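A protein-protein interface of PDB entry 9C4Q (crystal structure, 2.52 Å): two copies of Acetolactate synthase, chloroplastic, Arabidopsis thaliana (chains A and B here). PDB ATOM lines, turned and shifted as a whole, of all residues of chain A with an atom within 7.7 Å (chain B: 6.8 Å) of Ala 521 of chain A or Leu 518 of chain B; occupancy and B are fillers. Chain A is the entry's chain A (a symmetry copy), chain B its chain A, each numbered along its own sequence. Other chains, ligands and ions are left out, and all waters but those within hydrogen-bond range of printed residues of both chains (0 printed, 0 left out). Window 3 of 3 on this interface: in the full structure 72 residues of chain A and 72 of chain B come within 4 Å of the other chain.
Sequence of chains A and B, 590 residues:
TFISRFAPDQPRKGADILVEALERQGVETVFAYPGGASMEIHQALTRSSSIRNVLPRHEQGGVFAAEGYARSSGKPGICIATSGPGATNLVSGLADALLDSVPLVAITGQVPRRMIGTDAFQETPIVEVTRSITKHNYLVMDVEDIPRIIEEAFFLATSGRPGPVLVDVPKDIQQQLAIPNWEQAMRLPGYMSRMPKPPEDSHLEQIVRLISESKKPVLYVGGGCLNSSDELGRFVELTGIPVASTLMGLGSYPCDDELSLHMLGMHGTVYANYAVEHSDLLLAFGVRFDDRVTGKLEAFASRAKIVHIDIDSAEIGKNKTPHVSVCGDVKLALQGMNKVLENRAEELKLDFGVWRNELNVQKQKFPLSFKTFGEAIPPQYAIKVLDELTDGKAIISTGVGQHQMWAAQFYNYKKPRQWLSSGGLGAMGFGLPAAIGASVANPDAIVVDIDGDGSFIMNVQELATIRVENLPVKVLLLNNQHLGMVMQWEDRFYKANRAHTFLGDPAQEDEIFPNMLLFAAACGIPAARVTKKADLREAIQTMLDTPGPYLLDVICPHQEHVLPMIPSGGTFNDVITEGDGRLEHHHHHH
OD1 of Asn 515 of chain A sits at hydrogen-bond distance from N of Leu 517 of chain A (3.0 Å). The side-chain amide oxygen (OD1) of Asn 515 of chain B lies within hydrogen-bond range of the guanidinium group (NH2) of Arg 529 of chain B, 3.2 Å away. OD1 of Asn 515 of chain B lies within hydrogen-bond range of N of Leu 517 of chain B (3.0 Å).
N of Asn 515 of chain B is in hydrogen-bond range of O of Ala 522 of chain A (2.9 Å). The backbone carbonyl oxygen (O) of Ala 522 of chain B is in hydrogen-bond range of the backbone NH (N) of Asn 515 of chain A (2.9 Å).
Leu 518 of chain A touches Ala 522 of chain B, and with the chains exchanged Ala 522 of chain A touches Leu 518 of chain B. Phe 519 of chain A touches its own counterpart, Phe 519 of chain B. Phe 519 of chain A touches Ala 522 of chain B, and with the chains exchanged Ala 522 of chain A touches Phe 519 of chain B. Phe 519 of chain A touches Cys 523 of chain B, and with the chains exchanged Cys 523 of chain A touches Phe 519 of chain B. 12 positions are printed for both chains. Of the 13 pairs that touch across the chains among the printed residues, 12 have their exchanged pair printed and touching as well.
Printed residues of chain B that touch a printed residue of chain A: Phe 513, Asn 515, Leu 518, Phe 519, Ala 521, Ala 522 and Cys 523. Hydrophobic or aromatic side chains of chain B within 4 Å of the printed part of chain A: Phe 513, Leu 518, Phe 519, Ala 521 and Ala 522. Hydrophobic or aromatic side chains of chain A that line the printed part of chain B: Leu 518, Phe 519, Ala 521 and Ala 522.
Ala 521 of chain A touches one residue of chain B. Leu 518 of chain B touches just these residues of chain A: Leu 518, Ala 521 and Ala 522. Of the printed residues of chain B, Asn 515 of chain A touches Ala 522 (2.9 Å). Of the printed residues of chain A, Asn 515 of chain B touches Ala 522 (2.9 Å). Of the printed residues of chain A, Cys 523 of chain B touches Phe 519 (3.8 Å). Pro 526 of chain A touches none of the printed residues of chain B. The nearest residue of chain A that does not touch Leu 518 of chain B is Phe 519 of chain A (4.6 Å).
Among the printed residues, merely in contact across the chains: Leu 518 of chain A with Leu 518 of chain B (3.6 Å), Leu 518 of chain A with Ala 521 of chain B (3.6 Å), Leu 518 of chain A with Ala 522 of chain B (3.6 Å), Phe 519 of chain A with Phe 519 of chain B (3.3 Å), Phe 519 of chain A with Ala 522 of chain B (3.7 Å), Phe 519 of chain A with Cys 523 of chain B (3.8 Å), Ala 521 of chain A with Leu 518 of chain B (3.6 Å), Ala 522 of chain A with Leu 518 of chain B (3.6 Å), Ala 522 of chain A with Phe 519 of chain B (3.7 Å), Cys 523 of chain A with Phe 513 of chain B (3.4 Å) and Cys 523 of chain A with Phe 519 of chain B (3.8 Å).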
ATOM      1  N   LEU A 463       7.624 -38.345 -25.057  1.00  0.00           N
ATOM      2  CA  LEU A 463       7.704 -37.111 -25.833  1.00  0.00           C
ATOM      3  C   LEU A 463       9.144 -36.622 -25.928  1.00  0.00           C
ATOM      4  O   LEU A 463       9.561 -36.094 -26.965  1.00  0.00           O
ATOM      5  CB  LEU A 463       6.817 -36.030 -25.211  1.00  0.00           C
ATOM      6  CG  LEU A 463       5.301 -36.209 -25.266  1.00  0.00           C
ATOM      7  CD1 LEU A 463       4.610 -35.058 -24.548  1.00  0.00           C
ATOM      8  CD2 LEU A 463       4.822 -36.316 -26.704  1.00  0.00           C
ATOM      9  N   ASN A 515      -3.118 -30.100 -18.825  1.00  0.00           N
ATOM     10  CA  ASN A 515      -2.911 -29.348 -20.064  1.00  0.00           C
ATOM     11  C   ASN A 515      -1.847 -30.081 -20.874  1.00  0.00           C
ATOM     12  O   ASN A 515      -0.648 -29.860 -20.706  1.00  0.00           O
ATOM     13  CB  ASN A 515      -2.506 -27.909 -19.762  1.00  0.00           C
ATOM     14  CG  ASN A 515      -2.425 -27.038 -21.013  1.00  0.00           C
ATOM     15  OD1 ASN A 515      -2.345 -27.537 -22.135  1.00  0.00           O
ATOM     16  ND2 ASN A 515      -2.436 -25.726 -20.817  1.00  0.00           N
ATOM     17  N   MET A 516      -2.301 -30.950 -21.778  1.00  0.00           N
ATOM     18  CA  MET A 516      -1.378 -31.735 -22.588  1.00  0.00           C
ATOM     19  C   MET A 516      -0.502 -30.866 -23.480  1.00  0.00           C
ATOM     20  O   MET A 516       0.562 -31.320 -23.914  1.00  0.00           O
ATOM     21  CB  MET A 516      -2.158 -32.737 -23.435  1.00  0.00           C
ATOM     22  CG  MET A 516      -3.064 -33.651 -22.630  1.00  0.00           C
ATOM     23  SD  MET A 516      -2.164 -34.623 -21.412  1.00  0.00           S
ATOM     24  CE  MET A 516      -3.454 -35.732 -20.850  1.00  0.00           C
ATOM     25  N   LEU A 517      -0.920 -29.630 -23.765  1.00  0.00           N
ATOM     26  CA  LEU A 517      -0.099 -28.746 -24.584  1.00  0.00           C
ATOM     27  C   LEU A 517       1.216 -28.417 -23.889  1.00  0.00           C
ATOM     28  O   LEU A 517       2.251 -28.261 -24.548  1.00  0.00           O
ATOM     29  CB  LEU A 517      -0.863 -27.460 -24.911  1.00  0.00           C
ATOM     30  CG  LEU A 517      -2.227 -27.639 -25.577  1.00  0.00           C
ATOM     31  CD1 LEU A 517      -2.866 -26.293 -25.887  1.00  0.00           C
ATOM     32  CD2 LEU A 517      -2.094 -28.474 -26.840  1.00  0.00           C
ATOM     33  N   LEU A 518       1.197 -28.309 -22.558  1.00  0.00           N
ATOM     34  CA  LEU A 518       2.421 -27.986 -21.834  1.00  0.00           C
ATOM     35  C   LEU A 518       3.332 -29.198 -21.703  1.00  0.00           C
ATOM     36  O   LEU A 518       4.553 -29.039 -21.598  1.00  0.00           O
ATOM     37  CB  LEU A 518       2.079 -27.411 -20.460  1.00  0.00           C
ATOM     38  CG  LEU A 518       1.278 -26.110 -20.528  1.00  0.00           C
ATOM     39  CD1 LEU A 518       0.963 -25.589 -19.139  1.00  0.00           C
ATOM     40  CD2 LEU A 518       2.027 -25.067 -21.339  1.00  0.00           C
ATOM     41  N   PHE A 519       2.762 -30.407 -21.704  1.00  0.00           N
ATOM     42  CA  PHE A 519       3.577 -31.609 -21.835  1.00  0.00           C
ATOM     43  C   PHE A 519       4.371 -31.581 -23.135  1.00  0.00           C
ATOM     44  O   PHE A 519       5.576 -31.863 -23.149  1.00  0.00           O
ATOM     45  CB  PHE A 519       2.694 -32.858 -21.771  1.00  0.00           C
ATOM     46  CG  PHE A 519       2.259 -33.230 -20.379  1.00  0.00           C
ATOM     47  CD1 PHE A 519       3.190 -33.622 -19.434  1.00  0.00           C
ATOM     48  CD2 PHE A 519       0.923 -33.204 -20.019  1.00  0.00           C
ATOM     49  CE1 PHE A 519       2.803 -33.968 -18.153  1.00  0.00           C
ATOM     50  CE2 PHE A 519       0.527 -33.553 -18.736  1.00  0.00           C
ATOM     51  CZ  PHE A 519       1.469 -33.935 -17.804  1.00  0.00           C
ATOM     52  N   ALA A 520       3.707 -31.240 -24.242  1.00  0.00           N
ATOM     53  CA  ALA A 520       4.411 -31.087 -25.511  1.00  0.00           C
ATOM     54  C   ALA A 520       5.389 -29.921 -25.457  1.00  0.00           C
ATOM     55  O   ALA A 520       6.495 -30.002 -26.006  1.00  0.00           O
ATOM     56  CB  ALA A 520       3.405 -30.893 -26.648  1.00  0.00           C
ATOM     57  N   ALA A 521       5.003 -28.829 -24.793  1.00  0.00           N
ATOM     58  CA  ALA A 521       5.885 -27.671 -24.685  1.00  0.00           C
ATOM     59  C   ALA A 521       7.161 -28.016 -23.929  1.00  0.00           C
ATOM     60  O   ALA A 521       8.257 -27.602 -24.325  1.00  0.00           O
ATOM     61  CB  ALA A 521       5.152 -26.515 -24.003  1.00  0.00           C
ATOM     62  N   ALA A 522       7.036 -28.785 -22.842  1.00  0.00           N
ATOM     63  CA  ALA A 522       8.198 -29.170 -22.046  1.00  0.00           C
ATOM     64  C   ALA A 522       9.247 -29.887 -22.880  1.00  0.00           C
ATOM     65  O   ALA A 522      10.444 -29.795 -22.588  1.00  0.00           O
ATOM     66  CB  ALA A 522       7.763 -30.060 -20.880  1.00  0.00           C
ATOM     67  N   CYS A 523       8.822 -30.599 -23.923  1.00  0.00           N
ATOM     68  CA  CYS A 523       9.724 -31.356 -24.781  1.00  0.00           C
ATOM     69  C   CYS A 523       9.955 -30.678 -26.127  1.00  0.00           C
ATOM     70  O   CYS A 523      10.420 -31.322 -27.071  1.00  0.00           O
ATOM     71  CB  CYS A 523       9.185 -32.772 -24.979  1.00  0.00           C
ATOM     72  SG  CYS A 523       9.065 -33.738 -23.460  1.00  0.00           S
ATOM     73  N   GLY A 524       9.638 -29.389 -26.231  1.00  0.00           N
ATOM     74  CA  GLY A 524       9.874 -28.657 -27.463  1.00  0.00           C
ATOM     75  C   GLY A 524       9.104 -29.172 -28.660  1.00  0.00           C
ATOM     76  O   GLY A 524       9.626 -29.154 -29.779  1.00  0.00           O
ATOM     77  N   ILE A 525       7.874 -29.627 -28.457  1.00  0.00           N
ATOM     78  CA  ILE A 525       7.035 -30.184 -29.514  1.00  0.00           C
ATOM     79  C   ILE A 525       5.874 -29.222 -29.743  1.00  0.00           C
ATOM     80  O   ILE A 525       5.096 -28.969 -28.813  1.00  0.00           O
ATOM     81  CB  ILE A 525       6.528 -31.589 -29.154  1.00  0.00           C
ATOM     82  CG1 ILE A 525       7.702 -32.567 -29.090  1.00  0.00           C
ATOM     83  CG2 ILE A 525       5.471 -32.051 -30.146  1.00  0.00           C
ATOM     84  CD1 ILE A 525       7.319 -33.944 -28.602  1.00  0.00           C
ATOM     85  N   PRO A 526       5.724 -28.658 -30.943  1.00  0.00           N
ATOM     86  CA  PRO A 526       4.592 -27.760 -31.203  1.00  0.00           C
ATOM     87  C   PRO A 526       3.262 -28.459 -30.971  1.00  0.00           C
ATOM     88  O   PRO A 526       3.113 -29.657 -31.223  1.00  0.00           O
ATOM     89  CB  PRO A 526       4.775 -27.368 -32.675  1.00  0.00           C
ATOM     90  CG  PRO A 526       5.726 -28.378 -33.241  1.00  0.00           C
ATOM     91  CD  PRO A 526       6.615 -28.776 -32.108  1.00  0.00           C
ATOM     92  N   ALA A 527       2.291 -27.696 -30.476  1.00  0.00           N
ATOM     93  CA  ALA A 527       1.012 -28.267 -30.094  1.00  0.00           C
ATOM     94  C   ALA A 527      -0.086 -27.228 -30.262  1.00  0.00           C
ATOM     95  O   ALA A 527       0.175 -26.027 -30.373  1.00  0.00           O
ATOM     96  CB  ALA A 527       1.041 -28.791 -28.654  1.00  0.00           C
ATOM     97  N   LEU A 551       1.427 -32.245 -31.618  1.00  0.00           N
ATOM     98  CA  LEU A 551       0.338 -32.737 -30.785  1.00  0.00           C
ATOM     99  C   LEU A 551      -0.898 -31.875 -30.997  1.00  0.00           C
ATOM    100  O   LEU A 551      -0.840 -30.651 -30.848  1.00  0.00           O
ATOM    101  CB  LEU A 551       0.724 -32.735 -29.301  1.00  0.00           C
ATOM    102  CG  LEU A 551      -0.449 -32.751 -28.312  1.00  0.00           C
ATOM    103  CD1 LEU A 551      -1.246 -34.040 -28.396  1.00  0.00           C
ATOM    104  CD2 LEU A 551       0.032 -32.519 -26.884  1.00  0.00           C
ATOM    105  N   LEU B 463       2.283 -36.333 -11.418  1.00  0.00           N
ATOM    106  CA  LEU B 463       2.042 -34.930 -11.094  1.00  0.00           C
ATOM    107  C   LEU B 463       0.553 -34.610 -11.138  1.00  0.00           C
ATOM    108  O   LEU B 463       0.056 -33.820 -10.325  1.00  0.00           O
ATOM    109  CB  LEU B 463       2.810 -34.021 -12.056  1.00  0.00           C
ATOM    110  CG  LEU B 463       4.334 -33.992 -11.975  1.00  0.00           C
ATOM    111  CD1 LEU B 463       4.899 -33.071 -13.048  1.00  0.00           C
ATOM    112  CD2 LEU B 463       4.793 -33.559 -10.593  1.00  0.00           C
ATOM    113  N   PHE B 513      17.083 -29.807 -21.068  1.00  0.00           N
ATOM    114  CA  PHE B 513      16.033 -30.573 -21.719  1.00  0.00           C
ATOM    115  C   PHE B 513      15.754 -31.864 -20.960  1.00  0.00           C
ATOM    116  O   PHE B 513      16.688 -32.551 -20.528  1.00  0.00           O
ATOM    117  CB  PHE B 513      16.397 -30.905 -23.175  1.00  0.00           C
ATOM    118  CG  PHE B 513      15.311 -31.631 -23.913  1.00  0.00           C
ATOM    119  CD1 PHE B 513      14.282 -30.927 -24.523  1.00  0.00           C
ATOM    120  CD2 PHE B 513      15.301 -33.017 -23.976  1.00  0.00           C
ATOM    121  CE1 PHE B 513      13.269 -31.592 -25.199  1.00  0.00           C
ATOM    122  CE2 PHE B 513      14.289 -33.686 -24.646  1.00  0.00           C
ATOM    123  CZ  PHE B 513      13.274 -32.971 -25.261  1.00  0.00           C
ATOM    124  N   ASN B 515      12.106 -29.420 -20.244  1.00  0.00           N
ATOM    125  CA  ASN B 515      11.788 -28.331 -19.322  1.00  0.00           C
ATOM    126  C   ASN B 515      10.801 -28.872 -18.293  1.00  0.00           C
ATOM    127  O   ASN B 515       9.587 -28.862 -18.501  1.00  0.00           O
ATOM    128  CB  ASN B 515      11.223 -27.131 -20.075  1.00  0.00           C
ATOM    129  CG  ASN B 515      11.015 -25.911 -19.182  1.00  0.00           C
ATOM    130  OD1 ASN B 515      10.972 -26.015 -17.957  1.00  0.00           O
ATOM    131  ND2 ASN B 515      10.876 -24.746 -19.803  1.00  0.00           N
ATOM    132  N   MET B 516      11.335 -29.334 -17.162  1.00  0.00           N
ATOM    133  CA  MET B 516      10.494 -29.909 -16.119  1.00  0.00           C
ATOM    134  C   MET B 516       9.505 -28.901 -15.547  1.00  0.00           C
ATOM    135  O   MET B 516       8.492 -29.307 -14.967  1.00  0.00           O
ATOM    136  CB  MET B 516      11.370 -30.474 -15.003  1.00  0.00           C
ATOM    137  CG  MET B 516      12.392 -31.490 -15.477  1.00  0.00           C
ATOM    138  SD  MET B 516      11.637 -32.910 -16.286  1.00  0.00           S
ATOM    139  CE  MET B 516      13.059 -33.982 -16.474  1.00  0.00           C
ATOM    140  N   LEU B 517       9.770 -27.602 -15.696  1.00  0.00           N
ATOM    141  CA  LEU B 517       8.834 -26.598 -15.201  1.00  0.00           C
ATOM    142  C   LEU B 517       7.504 -26.675 -15.939  1.00  0.00           C
ATOM    143  O   LEU B 517       6.445 -26.432 -15.349  1.00  0.00           O
ATOM    144  CB  LEU B 517       9.436 -25.197 -15.335  1.00  0.00           C
ATOM    145  CG  LEU B 517      10.797 -24.983 -14.674  1.00  0.00           C
ATOM    146  CD1 LEU B 517      11.267 -23.546 -14.841  1.00  0.00           C
ATOM    147  CD2 LEU B 517      10.737 -25.362 -13.204  1.00  0.00           C
ATOM    148  N   LEU B 518       7.536 -27.013 -17.232  1.00  0.00           N
ATOM    149  CA  LEU B 518       6.298 -27.094 -17.996  1.00  0.00           C
ATOM    150  C   LEU B 518       5.538 -28.379 -17.699  1.00  0.00           C
ATOM    151  O   LEU B 518       4.309 -28.408 -17.826  1.00  0.00           O
ATOM    152  CB  LEU B 518       6.598 -26.971 -19.490  1.00  0.00           C
ATOM    153  CG  LEU B 518       7.239 -25.637 -19.873  1.00  0.00           C
ATOM    154  CD1 LEU B 518       7.518 -25.573 -21.363  1.00  0.00           C
ATOM    155  CD2 LEU B 518       6.356 -24.479 -19.438  1.00  0.00           C
ATOM    156  N   PHE B 519       6.246 -29.443 -17.310  1.00  0.00           N
ATOM    157  CA  PHE B 519       5.575 -30.621 -16.771  1.00  0.00           C
ATOM    158  C   PHE B 519       4.756 -30.257 -15.539  1.00  0.00           C
ATOM    159  O   PHE B 519       3.594 -30.657 -15.407  1.00  0.00           O
ATOM    160  CB  PHE B 519       6.599 -31.708 -16.436  1.00  0.00           C
ATOM    161  CG  PHE B 519       7.103 -32.467 -17.634  1.00  0.00           C
ATOM    162  CD1 PHE B 519       6.243 -33.256 -18.376  1.00  0.00           C
ATOM    163  CD2 PHE B 519       8.434 -32.404 -18.009  1.00  0.00           C
ATOM    164  CE1 PHE B 519       6.694 -33.958 -19.479  1.00  0.00           C
ATOM    165  CE2 PHE B 519       8.894 -33.110 -19.111  1.00  0.00           C
ATOM    166  CZ  PHE B 519       8.022 -33.887 -19.844  1.00  0.00           C
ATOM    167  N   ALA B 520       5.354 -29.492 -14.620  1.00  0.00           N
ATOM    168  CA  ALA B 520       4.613 -29.011 -13.460  1.00  0.00           C
ATOM    169  C   ALA B 520       3.504 -28.053 -13.878  1.00  0.00           C
ATOM    170  O   ALA B 520       2.406 -28.076 -13.311  1.00  0.00           O
ATOM    171  CB  ALA B 520       5.565 -28.335 -12.472  1.00  0.00           C
ATOM    172  N   ALA B 521       3.773 -27.204 -14.873  1.00  0.00           N
ATOM    173  CA  ALA B 521       2.764 -26.260 -15.342  1.00  0.00           C
ATOM    174  C   ALA B 521       1.553 -26.984 -15.915  1.00  0.00           C
ATOM    175  O   ALA B 521       0.408 -26.594 -15.656  1.00  0.00           O
ATOM    176  CB  ALA B 521       3.371 -25.318 -16.383  1.00  0.00           C
ATOM    177  N   ALA B 522       1.789 -28.049 -16.688  1.00  0.00           N
ATOM    178  CA  ALA B 522       0.697 -28.809 -17.288  1.00  0.00           C
ATOM    179  C   ALA B 522      -0.277 -29.327 -16.242  1.00  0.00           C
ATOM    180  O   ALA B 522      -1.471 -29.479 -16.524  1.00  0.00           O
ATOM    181  CB  ALA B 522       1.255 -29.979 -18.101  1.00  0.00           C
ATOM    182  N   CYS B 523       0.207 -29.599 -15.031  1.00  0.00           N
ATOM    183  CA  CYS B 523      -0.618 -30.128 -13.954  1.00  0.00           C
ATOM    184  C   CYS B 523      -0.953 -29.075 -12.904  1.00  0.00           C
ATOM    185  O   CYS B 523      -1.358 -29.419 -11.791  1.00  0.00           O
ATOM    186  CB  CYS B 523       0.080 -31.325 -13.309  1.00  0.00           C
ATOM    187  SG  CYS B 523       0.342 -32.719 -14.423  1.00  0.00           S
ATOM    188  N   ALA B 527       6.219 -23.943  -9.943  1.00  0.00           N
ATOM    189  CA  ALA B 527       7.565 -24.454 -10.140  1.00  0.00           C
ATOM    190  C   ALA B 527       8.529 -23.297 -10.349  1.00  0.00           C
ATOM    191  O   ALA B 527       8.127 -22.167 -10.636  1.00  0.00           O
ATOM    192  CB  ALA B 527       7.626 -25.425 -11.324  1.00  0.00           C
ATOM    193  N   ARG B 529      13.098 -22.681 -11.324  1.00  0.00           N
ATOM    194  CA  ARG B 529      14.428 -23.209 -11.585  1.00  0.00           C
ATOM    195  C   ARG B 529      15.472 -22.303 -10.946  1.00  0.00           C
ATOM    196  O   ARG B 529      15.353 -21.075 -10.990  1.00  0.00           O
ATOM    197  CB  ARG B 529      14.698 -23.338 -13.091  1.00  0.00           C
ATOM    198  CG  ARG B 529      16.087 -23.871 -13.423  1.00  0.00           C
ATOM    199  CD  ARG B 529      16.291 -23.999 -14.919  1.00  0.00           C
ATOM    200  NE  ARG B 529      15.269 -24.845 -15.520  1.00  0.00           N
ATOM    201  CZ  ARG B 529      15.093 -24.996 -16.825  1.00  0.00           C
ATOM    202  NH1 ARG B 529      15.863 -24.372 -17.704  1.00  0.00           N
ATOM    203  NH2 ARG B 529      14.117 -25.789 -17.261  1.00  0.00           N
ATOM    204  N   LEU B 551       7.588 -27.721  -7.375  1.00  0.00           N
ATOM    205  CA  LEU B 551       8.744 -28.331  -8.020  1.00  0.00           C
ATOM    206  C   LEU B 551       9.865 -27.308  -8.131  1.00  0.00           C
ATOM    207  O   LEU B 551       9.667 -26.219  -8.677  1.00  0.00           O
ATOM    208  CB  LEU B 551       8.391 -28.866  -9.413  1.00  0.00           C
ATOM    209  CG  LEU B 551       9.577 -29.072 -10.364  1.00  0.00           C
ATOM    210  CD1 LEU B 551      10.518 -30.157  -9.873  1.00  0.00           C
ATOM    211  CD2 LEU B 551       9.100 -29.384 -11.777  1.00  0.00           C
